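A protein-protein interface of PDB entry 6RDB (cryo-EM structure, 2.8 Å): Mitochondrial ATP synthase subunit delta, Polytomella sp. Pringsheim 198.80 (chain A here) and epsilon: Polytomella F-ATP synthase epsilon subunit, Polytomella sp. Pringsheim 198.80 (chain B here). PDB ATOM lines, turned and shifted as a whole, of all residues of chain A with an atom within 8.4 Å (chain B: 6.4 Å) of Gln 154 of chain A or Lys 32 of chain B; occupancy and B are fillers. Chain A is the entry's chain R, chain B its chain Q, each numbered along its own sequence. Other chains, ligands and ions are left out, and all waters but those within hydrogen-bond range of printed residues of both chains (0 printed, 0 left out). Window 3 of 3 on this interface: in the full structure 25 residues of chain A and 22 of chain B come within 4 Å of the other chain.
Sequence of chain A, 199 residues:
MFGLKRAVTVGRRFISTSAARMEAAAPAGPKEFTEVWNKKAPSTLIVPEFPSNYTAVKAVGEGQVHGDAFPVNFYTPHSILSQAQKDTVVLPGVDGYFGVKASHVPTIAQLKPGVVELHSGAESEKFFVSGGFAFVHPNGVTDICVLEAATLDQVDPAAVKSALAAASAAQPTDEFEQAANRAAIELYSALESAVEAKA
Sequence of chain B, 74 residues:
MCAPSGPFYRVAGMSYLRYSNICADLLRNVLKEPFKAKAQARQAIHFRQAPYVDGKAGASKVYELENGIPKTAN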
ATOM      1  N   HIS A  78      11.216   4.058  15.733  1.00  0.00           N
ATOM      2  CA  HIS A  78      12.196   4.386  14.715  1.00  0.00           C
ATOM      3  C   HIS A  78      11.611   4.480  13.312  1.00  0.00           C
ATOM      4  O   HIS A  78      12.373   4.666  12.359  1.00  0.00           O
ATOM      5  CB  HIS A  78      13.329   3.354  14.736  1.00  0.00           C
ATOM      6  CG  HIS A  78      12.855   1.943  14.892  1.00  0.00           C
ATOM      7  ND1 HIS A  78      12.608   1.375  16.123  1.00  0.00           N
ATOM      8  CD2 HIS A  78      12.593   0.984  13.975  1.00  0.00           C
ATOM      9  CE1 HIS A  78      12.200   0.131  15.956  1.00  0.00           C
ATOM     10  NE2 HIS A  78      12.190  -0.134  14.662  1.00  0.00           N
ATOM     11  N   LEU A  81       5.493   3.458   9.664  1.00  0.00           N
ATOM     12  CA  LEU A  81       5.371   2.400   8.669  1.00  0.00           C
ATOM     13  C   LEU A  81       4.191   2.618   7.737  1.00  0.00           C
ATOM     14  O   LEU A  81       4.262   2.252   6.560  1.00  0.00           O
ATOM     15  CB  LEU A  81       5.259   1.046   9.356  1.00  0.00           C
ATOM     16  CG  LEU A  81       6.571   0.591   9.976  1.00  0.00           C
ATOM     17  CD1 LEU A  81       6.281  -0.426  11.018  1.00  0.00           C
ATOM     18  CD2 LEU A  81       7.487   0.011   8.921  1.00  0.00           C
ATOM     19  N   LYS A 126       1.728  -7.694   5.759  1.00  0.00           N
ATOM     20  CA  LYS A 126       1.735  -8.372   7.050  1.00  0.00           C
ATOM     21  C   LYS A 126       2.992  -7.973   7.808  1.00  0.00           C
ATOM     22  O   LYS A 126       4.100  -8.365   7.428  1.00  0.00           O
ATOM     23  CB  LYS A 126       1.673  -9.889   6.878  1.00  0.00           C
ATOM     24  CG  LYS A 126       0.729 -10.380   5.794  1.00  0.00           C
ATOM     25  CD  LYS A 126      -0.720 -10.076   6.122  1.00  0.00           C
ATOM     26  CE  LYS A 126      -1.659 -10.789   5.166  1.00  0.00           C
ATOM     27  NZ  LYS A 126      -1.578 -12.266   5.326  1.00  0.00           N
ATOM     28  N   PHE A 127       2.820  -7.201   8.875  1.00  0.00           N
ATOM     29  CA  PHE A 127       3.900  -6.876   9.793  1.00  0.00           C
ATOM     30  C   PHE A 127       3.727  -7.686  11.065  1.00  0.00           C
ATOM     31  O   PHE A 127       2.659  -7.656  11.680  1.00  0.00           O
ATOM     32  CB  PHE A 127       3.909  -5.388  10.140  1.00  0.00           C
ATOM     33  CG  PHE A 127       4.146  -4.495   8.974  1.00  0.00           C
ATOM     34  CD1 PHE A 127       5.433  -4.215   8.556  1.00  0.00           C
ATOM     35  CD2 PHE A 127       3.082  -3.926   8.301  1.00  0.00           C
ATOM     36  CE1 PHE A 127       5.652  -3.388   7.479  1.00  0.00           C
ATOM     37  CE2 PHE A 127       3.291  -3.097   7.223  1.00  0.00           C
ATOM     38  CZ  PHE A 127       4.577  -2.828   6.810  1.00  0.00           C
ATOM     39  N   PHE A 128       4.776  -8.391  11.469  1.00  0.00           N
ATOM     40  CA  PHE A 128       4.789  -9.065  12.757  1.00  0.00           C
ATOM     41  C   PHE A 128       5.372  -8.121  13.797  1.00  0.00           C
ATOM     42  O   PHE A 128       6.513  -7.670  13.663  1.00  0.00           O
ATOM     43  CB  PHE A 128       5.605 -10.353  12.693  1.00  0.00           C
ATOM     44  CG  PHE A 128       5.688 -11.074  14.001  1.00  0.00           C
ATOM     45  CD1 PHE A 128       4.616 -11.810  14.469  1.00  0.00           C
ATOM     46  CD2 PHE A 128       6.838 -11.013  14.766  1.00  0.00           C
ATOM     47  CE1 PHE A 128       4.690 -12.471  15.673  1.00  0.00           C
ATOM     48  CE2 PHE A 128       6.918 -11.673  15.969  1.00  0.00           C
ATOM     49  CZ  PHE A 128       5.842 -12.402  16.424  1.00  0.00           C
ATOM     50  N   GLU A 148       8.929  -2.947  17.959  1.00  0.00           N
ATOM     51  CA  GLU A 148       9.617  -3.555  16.826  1.00  0.00           C
ATOM     52  C   GLU A 148       8.567  -4.192  15.933  1.00  0.00           C
ATOM     53  O   GLU A 148       7.890  -5.138  16.345  1.00  0.00           O
ATOM     54  CB  GLU A 148      10.648  -4.582  17.284  1.00  0.00           C
ATOM     55  CG  GLU A 148      11.652  -4.959  16.208  1.00  0.00           C
ATOM     56  CD  GLU A 148      12.686  -3.875  15.957  1.00  0.00           C
ATOM     57  OE1 GLU A 148      12.943  -3.066  16.874  1.00  0.00           O
ATOM     58  OE2 GLU A 148      13.250  -3.834  14.844  1.00  0.00           O
ATOM     59  N   ALA A 149       8.426  -3.675  14.720  1.00  0.00           N
ATOM     60  CA  ALA A 149       7.430  -4.165  13.777  1.00  0.00           C
ATOM     61  C   ALA A 149       8.142  -4.589  12.500  1.00  0.00           C
ATOM     62  O   ALA A 149       8.223  -3.825  11.536  1.00  0.00           O
ATOM     63  CB  ALA A 149       6.403  -3.117  13.504  1.00  0.00           C
ATOM     64  N   ALA A 150       8.635  -5.822  12.491  1.00  0.00           N
ATOM     65  CA  ALA A 150       9.295  -6.377  11.322  1.00  0.00           C
ATOM     66  C   ALA A 150       8.267  -6.994  10.390  1.00  0.00           C
ATOM     67  O   ALA A 150       7.309  -7.630  10.835  1.00  0.00           O
ATOM     68  CB  ALA A 150      10.323  -7.430  11.731  1.00  0.00           C
ATOM     69  N   THR A 151       8.463  -6.794   9.094  1.00  0.00           N
ATOM     70  CA  THR A 151       7.657  -7.517   8.129  1.00  0.00           C
ATOM     71  C   THR A 151       8.132  -8.965   8.056  1.00  0.00           C
ATOM     72  O   THR A 151       9.249  -9.303   8.455  1.00  0.00           O
ATOM     73  CB  THR A 151       7.716  -6.842   6.753  1.00  0.00           C
ATOM     74  OG1 THR A 151       6.671  -7.357   5.919  1.00  0.00           O
ATOM     75  CG2 THR A 151       9.069  -7.070   6.080  1.00  0.00           C
ATOM     76  N   LEU A 152       7.258  -9.831   7.551  1.00  0.00           N
ATOM     77  CA  LEU A 152       7.527 -11.262   7.546  1.00  0.00           C
ATOM     78  C   LEU A 152       8.486 -11.691   6.445  1.00  0.00           C
ATOM     79  O   LEU A 152       8.888 -12.859   6.419  1.00  0.00           O
ATOM     80  CB  LEU A 152       6.205 -12.019   7.440  1.00  0.00           C
ATOM     81  CG  LEU A 152       5.455 -11.895   8.765  1.00  0.00           C
ATOM     82  CD1 LEU A 152       4.019 -12.309   8.648  1.00  0.00           C
ATOM     83  CD2 LEU A 152       6.158 -12.751   9.807  1.00  0.00           C
ATOM     84  N   ASP A 153       8.868 -10.780   5.551  1.00  0.00           N
ATOM     85  CA  ASP A 153       9.873 -11.081   4.543  1.00  0.00           C
ATOM     86  C   ASP A 153      11.273 -11.181   5.131  1.00  0.00           C
ATOM     87  O   ASP A 153      12.112 -11.899   4.579  1.00  0.00           O
ATOM     88  CB  ASP A 153       9.856 -10.002   3.462  1.00  0.00           C
ATOM     89  CG  ASP A 153       8.472  -9.764   2.898  1.00  0.00           C
ATOM     90  OD1 ASP A 153       7.533 -10.482   3.304  1.00  0.00           O
ATOM     91  OD2 ASP A 153       8.321  -8.847   2.065  1.00  0.00           O
ATOM     92  N   GLN A 154      11.537 -10.488   6.241  1.00  0.00           N
ATOM     93  CA  GLN A 154      12.872 -10.410   6.823  1.00  0.00           C
ATOM     94  C   GLN A 154      12.964 -11.124   8.167  1.00  0.00           C
ATOM     95  O   GLN A 154      13.816 -10.778   8.991  1.00  0.00           O
ATOM     96  CB  GLN A 154      13.303  -8.953   6.968  1.00  0.00           C
ATOM     97  CG  GLN A 154      12.338  -8.086   7.750  1.00  0.00           C
ATOM     98  CD  GLN A 154      12.625  -6.608   7.586  1.00  0.00           C
ATOM     99  OE1 GLN A 154      13.174  -6.180   6.572  1.00  0.00           O
ATOM    100  NE2 GLN A 154      12.264  -5.821   8.590  1.00  0.00           N
ATOM    101  N   VAL A 155      12.108 -12.102   8.408  1.00  0.00           N
ATOM    102  CA  VAL A 155      12.229 -12.974   9.569  1.00  0.00           C
ATOM    103  C   VAL A 155      12.731 -14.323   9.078  1.00  0.00           C
ATOM    104  O   VAL A 155      12.401 -14.763   7.971  1.00  0.00           O
ATOM    105  CB  VAL A 155      10.883 -13.100  10.319  1.00  0.00           C
ATOM    106  CG1 VAL A 155      11.072 -13.715  11.700  1.00  0.00           C
ATOM    107  CG2 VAL A 155      10.218 -11.743  10.439  1.00  0.00           C
ATOM    108  N   ASP A 156      13.559 -14.988   9.895  1.00  0.00           N
ATOM    109  CA  ASP A 156      13.984 -16.305   9.451  1.00  0.00           C
ATOM    110  C   ASP A 156      13.200 -17.398  10.172  1.00  0.00           C
ATOM    111  O   ASP A 156      12.948 -17.294  11.378  1.00  0.00           O
ATOM    112  CB  ASP A 156      15.491 -16.521   9.664  1.00  0.00           C
ATOM    113  CG  ASP A 156      15.912 -16.397  11.116  1.00  0.00           C
ATOM    114  OD1 ASP A 156      16.425 -15.322  11.488  1.00  0.00           O
ATOM    115  OD2 ASP A 156      15.764 -17.373  11.880  1.00  0.00           O
ATOM    116  N   PRO A 157      12.766 -18.435   9.454  1.00  0.00           N
ATOM    117  CA  PRO A 157      12.121 -19.577  10.111  1.00  0.00           C
ATOM    118  C   PRO A 157      13.090 -20.593  10.695  1.00  0.00           C
ATOM    119  O   PRO A 157      12.639 -21.623  11.206  1.00  0.00           O
ATOM    120  CB  PRO A 157      11.293 -20.194   8.977  1.00  0.00           C
ATOM    121  CG  PRO A 157      12.044 -19.845   7.746  1.00  0.00           C
ATOM    122  CD  PRO A 157      12.628 -18.488   7.988  1.00  0.00           C
ATOM    123  N   ALA A 158      14.395 -20.338  10.652  1.00  0.00           N
ATOM    124  CA  ALA A 158      15.364 -21.314  11.134  1.00  0.00           C
ATOM    125  C   ALA A 158      15.753 -21.076  12.589  1.00  0.00           C
ATOM    126  O   ALA A 158      15.526 -21.937  13.444  1.00  0.00           O
ATOM    127  CB  ALA A 158      16.612 -21.296  10.245  1.00  0.00           C
ATOM    128  N   LEU A 191       5.218 -16.375  16.375  1.00  0.00           N
ATOM    129  CA  LEU A 191       5.997 -16.106  15.174  1.00  0.00           C
ATOM    130  C   LEU A 191       6.106 -17.333  14.280  1.00  0.00           C
ATOM    131  O   LEU A 191       5.999 -17.209  13.054  1.00  0.00           O
ATOM    132  CB  LEU A 191       7.392 -15.608  15.561  1.00  0.00           C
ATOM    133  CG  LEU A 191       8.365 -15.175  14.465  1.00  0.00           C
ATOM    134  CD1 LEU A 191       7.697 -14.266  13.444  1.00  0.00           C
ATOM    135  CD2 LEU A 191       9.564 -14.496  15.092  1.00  0.00           C
ATOM    136  N   ARG B  28      14.426  -8.918  17.171  1.00  0.00           N
ATOM    137  CA  ARG B  28      15.574  -8.559  16.346  1.00  0.00           C
ATOM    138  C   ARG B  28      16.594  -9.684  16.232  1.00  0.00           C
ATOM    139  O   ARG B  28      17.311  -9.747  15.231  1.00  0.00           O
ATOM    140  CB  ARG B  28      16.260  -7.310  16.897  1.00  0.00           C
ATOM    141  CG  ARG B  28      15.390  -6.069  16.927  1.00  0.00           C
ATOM    142  CD  ARG B  28      16.157  -4.886  17.482  1.00  0.00           C
ATOM    143  NE  ARG B  28      15.266  -3.825  17.935  1.00  0.00           N
ATOM    144  CZ  ARG B  28      15.031  -3.546  19.211  1.00  0.00           C
ATOM    145  NH1 ARG B  28      15.625  -4.251  20.162  1.00  0.00           N
ATOM    146  NH2 ARG B  28      14.200  -2.569  19.537  1.00  0.00           N
ATOM    147  N   VAL B  30      15.945 -12.736  15.670  1.00  0.00           N
ATOM    148  CA  VAL B  30      15.492 -13.667  14.650  1.00  0.00           C
ATOM    149  C   VAL B  30      15.109 -12.944  13.355  1.00  0.00           C
ATOM    150  O   VAL B  30      14.249 -13.415  12.615  1.00  0.00           O
ATOM    151  CB  VAL B  30      14.348 -14.553  15.173  1.00  0.00           C
ATOM    152  CG1 VAL B  30      14.858 -15.478  16.262  1.00  0.00           C
ATOM    153  CG2 VAL B  30      13.227 -13.712  15.725  1.00  0.00           C
ATOM    154  N   LEU B  31      15.742 -11.813  13.059  1.00  0.00           N
ATOM    155  CA  LEU B  31      15.619 -11.205  11.742  1.00  0.00           C
ATOM    156  C   LEU B  31      16.661 -11.744  10.766  1.00  0.00           C
ATOM    157  O   LEU B  31      17.694 -12.297  11.152  1.00  0.00           O
ATOM    158  CB  LEU B  31      15.731  -9.677  11.801  1.00  0.00           C
ATOM    159  CG  LEU B  31      14.460  -8.821  11.702  1.00  0.00           C
ATOM    160  CD1 LEU B  31      13.548  -8.951  12.888  1.00  0.00           C
ATOM    161  CD2 LEU B  31      14.818  -7.354  11.470  1.00  0.00           C
ATOM    162  N   LYS B  32      16.354 -11.573   9.482  1.00  0.00           N
ATOM    163  CA  LYS B  32      17.261 -11.910   8.397  1.00  0.00           C
ATOM    164  C   LYS B  32      18.476 -10.986   8.418  1.00  0.00           C
ATOM    165  O   LYS B  32      18.366  -9.793   8.711  1.00  0.00           O
ATOM    166  CB  LYS B  32      16.521 -11.796   7.062  1.00  0.00           C
ATOM    167  CG  LYS B  32      17.254 -12.330   5.847  1.00  0.00           C
ATOM    168  CD  LYS B  32      17.475 -13.829   5.957  1.00  0.00           C
ATOM    169  CE  LYS B  32      16.151 -14.584   6.007  1.00  0.00           C
ATOM    170  NZ  LYS B  32      15.385 -14.504   4.734  1.00  0.00           N
ATOM    171  N   GLU B  33      19.639 -11.554   8.089  1.00  0.00           N
ATOM    172  CA  GLU B  33      20.906 -10.837   8.243  1.00  0.00           C
ATOM    173  C   GLU B  33      21.095  -9.590   7.368  1.00  0.00           C
ATOM    174  O   GLU B  33      21.820  -8.685   7.818  1.00  0.00           O
ATOM    175  CB  GLU B  33      22.068 -11.824   8.038  1.00  0.00           C
ATOM    176  CG  GLU B  33      23.379 -11.398   8.685  1.00  0.00           C
ATOM    177  CD  GLU B  33      23.211 -10.955  10.128  1.00  0.00           C
ATOM    178  OE1 GLU B  33      22.639 -11.722  10.929  1.00  0.00           O
ATOM    179  OE2 GLU B  33      23.650  -9.834  10.461  1.00  0.00           O
ATOM    180  N   PRO B  34      20.510  -9.450   6.167  1.00  0.00           N
ATOM    181  CA  PRO B  34      20.465  -8.111   5.546  1.00  0.00           C
ATOM    182  C   PRO B  34      19.689  -7.061   6.335  1.00  0.00           C
ATOM    183  O   PRO B  34      19.833  -5.867   6.044  1.00  0.00           O
ATOM    184  CB  PRO B  34      19.804  -8.380   4.192  1.00  0.00           C
ATOM    185  CG  PRO B  34      20.269  -9.720   3.842  1.00  0.00           C
ATOM    186  CD  PRO B  34      20.358 -10.493   5.128  1.00  0.00           C
ATOM    187  N   PHE B  35      18.874  -7.455   7.315  1.00  0.00           N
ATOM    188  CA  PHE B  35      18.156  -6.512   8.154  1.00  0.00           C
ATOM    189  C   PHE B  35      18.388  -6.726   9.643  1.00  0.00           C
ATOM    190  O   PHE B  35      17.860  -5.954  10.449  1.00  0.00           O
ATOM    191  CB  PHE B  35      16.656  -6.578   7.849  1.00  0.00           C
ATOM    192  CG  PHE B  35      16.323  -6.269   6.422  1.00  0.00           C
ATOM    193  CD1 PHE B  35      16.213  -4.954   5.996  1.00  0.00           C
ATOM    194  CD2 PHE B  35      16.130  -7.287   5.503  1.00  0.00           C
ATOM    195  CE1 PHE B  35      15.908  -4.660   4.679  1.00  0.00           C
ATOM    196  CE2 PHE B  35      15.825  -7.003   4.186  1.00  0.00           C
ATOM    197  CZ  PHE B  35      15.713  -5.686   3.773  1.00  0.00           C
ATOM    198  N   LYS B  36      19.160  -7.742  10.034  1.00  0.00           N
ATOM    199  CA  LYS B  36      19.402  -7.994  11.451  1.00  0.00           C
ATOM    200  C   LYS B  36      20.491  -7.085  12.010  1.00  0.00           C
ATOM    201  O   LYS B  36      20.410  -6.651  13.164  1.00  0.00           O
ATOM    202  CB  LYS B  36      19.777  -9.461  11.664  1.00  0.00           C
ATOM    203  CG  LYS B  36      19.895  -9.877  13.122  1.00  0.00           C
ATOM    204  CD  LYS B  36      20.282 -11.335  13.254  1.00  0.00           C
ATOM    205  CE  LYS B  36      20.651 -11.679  14.685  1.00  0.00           C
ATOM    206  NZ  LYS B  36      21.777 -10.842  15.176  1.00  0.00           N
ATOM    207  N   ALA B  37      21.512  -6.779  11.208  1.00  0.00           N
ATOM    208  CA  ALA B  37      22.614  -5.953  11.691  1.00  0.00           C
ATOM    209  C   ALA B  37      22.239  -4.482  11.766  1.00  0.00           C
ATOM    210  O   ALA B  37      22.764  -3.759  12.620  1.00  0.00           O
ATOM    211  CB  ALA B  37      23.844  -6.135  10.802  1.00  0.00           C
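The backbone NH (N) of Phe 128 of chain A is in hydrogen-bond range of the backbone carbonyl oxygen (O) of Ala 150 of chain A (2.7 Å).
OD2 of Asp 156 of chain A lies close to N of Ala 158 of chain A (3.5 Å).
Lys 32 of chain B touches one residue of chain A.
Leu 31 of chain B touches three residues of chain A.
Phe 35 of chain B touches just one residue of chain A: Gln 154 (3.2 Å).
Printed residues of chain A within 4 Å of Arg 28 of chain B: Glu 148 (2.7 Å).
Printed residues of chain B within 4 Å of Glu 148 of chain A: Arg 28 (2.7 Å).
Printed residues of chain A within 4 Å of Val 30 of chain B: Val 155, Asp 156 and Leu 191.
Of the printed residues of chain B, Leu 191 of chain A touches Val 30.
Ala 158 of chain A touches none of the printed residues of chain B.
The nearest residue of chain B that does not touch Gln 154 of chain A is Val 30 of chain B (4.5 Å).
The nearest printed residue of chain A that does not touch Lys 32 of chain B is Asp 153 of chain A (4.2 Å).
The nearest printed residue of chain B that does not touch Leu 191 of chain A is Leu 31 of chain B (7.0 Å).
Among the printed residues, pairs that only touch across the chains: Gln 154 of chain A with Phe 35 of chain B, Gln 154 of chain A with Leu 31 of chain B, Val 155 of chain A with Val 30 of chain B, Ala 150 of chain A with Leu 31 of chain B and Leu 191 of chain A with Val 30 of chain B.
Of the 9 printed residues of chain B, 5 touch a printed residue of chain A.
Printed residues of chain B that touch a printed residue of chain A: Arg 28, Val 30, Leu 31, Lys 32 and Phe 35.
Hydrophobic or aromatic side chains of chain B within 4 Å of the printed part of chain A: Val 30, Leu 31 and Phe 35.
Of the 17 printed residues of chain A, 6 touch a printed residue of chain B.
Printed residues of chain A that touch a printed residue of chain B: Glu 148, Ala 150, Gln 154, Val 155, Asp 156 and Leu 191.
Hydrophobic or aromatic side chains of chain A that line the printed part of chain B: Ala 150, Val 155 and Leu 191.
O of Gln 154 of chain A is in hydrogen-bond range of N of Lys 32 of chain B, at 2.7 Å.
The backbone carbonyl oxygen (O) of Leu 31 of chain B sits close to the side-chain carboxylate (OD1) of Asp 156 of chain A (3.3 Å).
NE of Arg 28 of chain B is in salt-bridge range of OE1 of Glu 148 of chain A, at 2.7 Å.
The backbone carbonyl oxygen of Val 30 of chain B sits at hydrogen-bond distance from the backbone NH of Asp 156 of chain A, at 3.2 Å.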
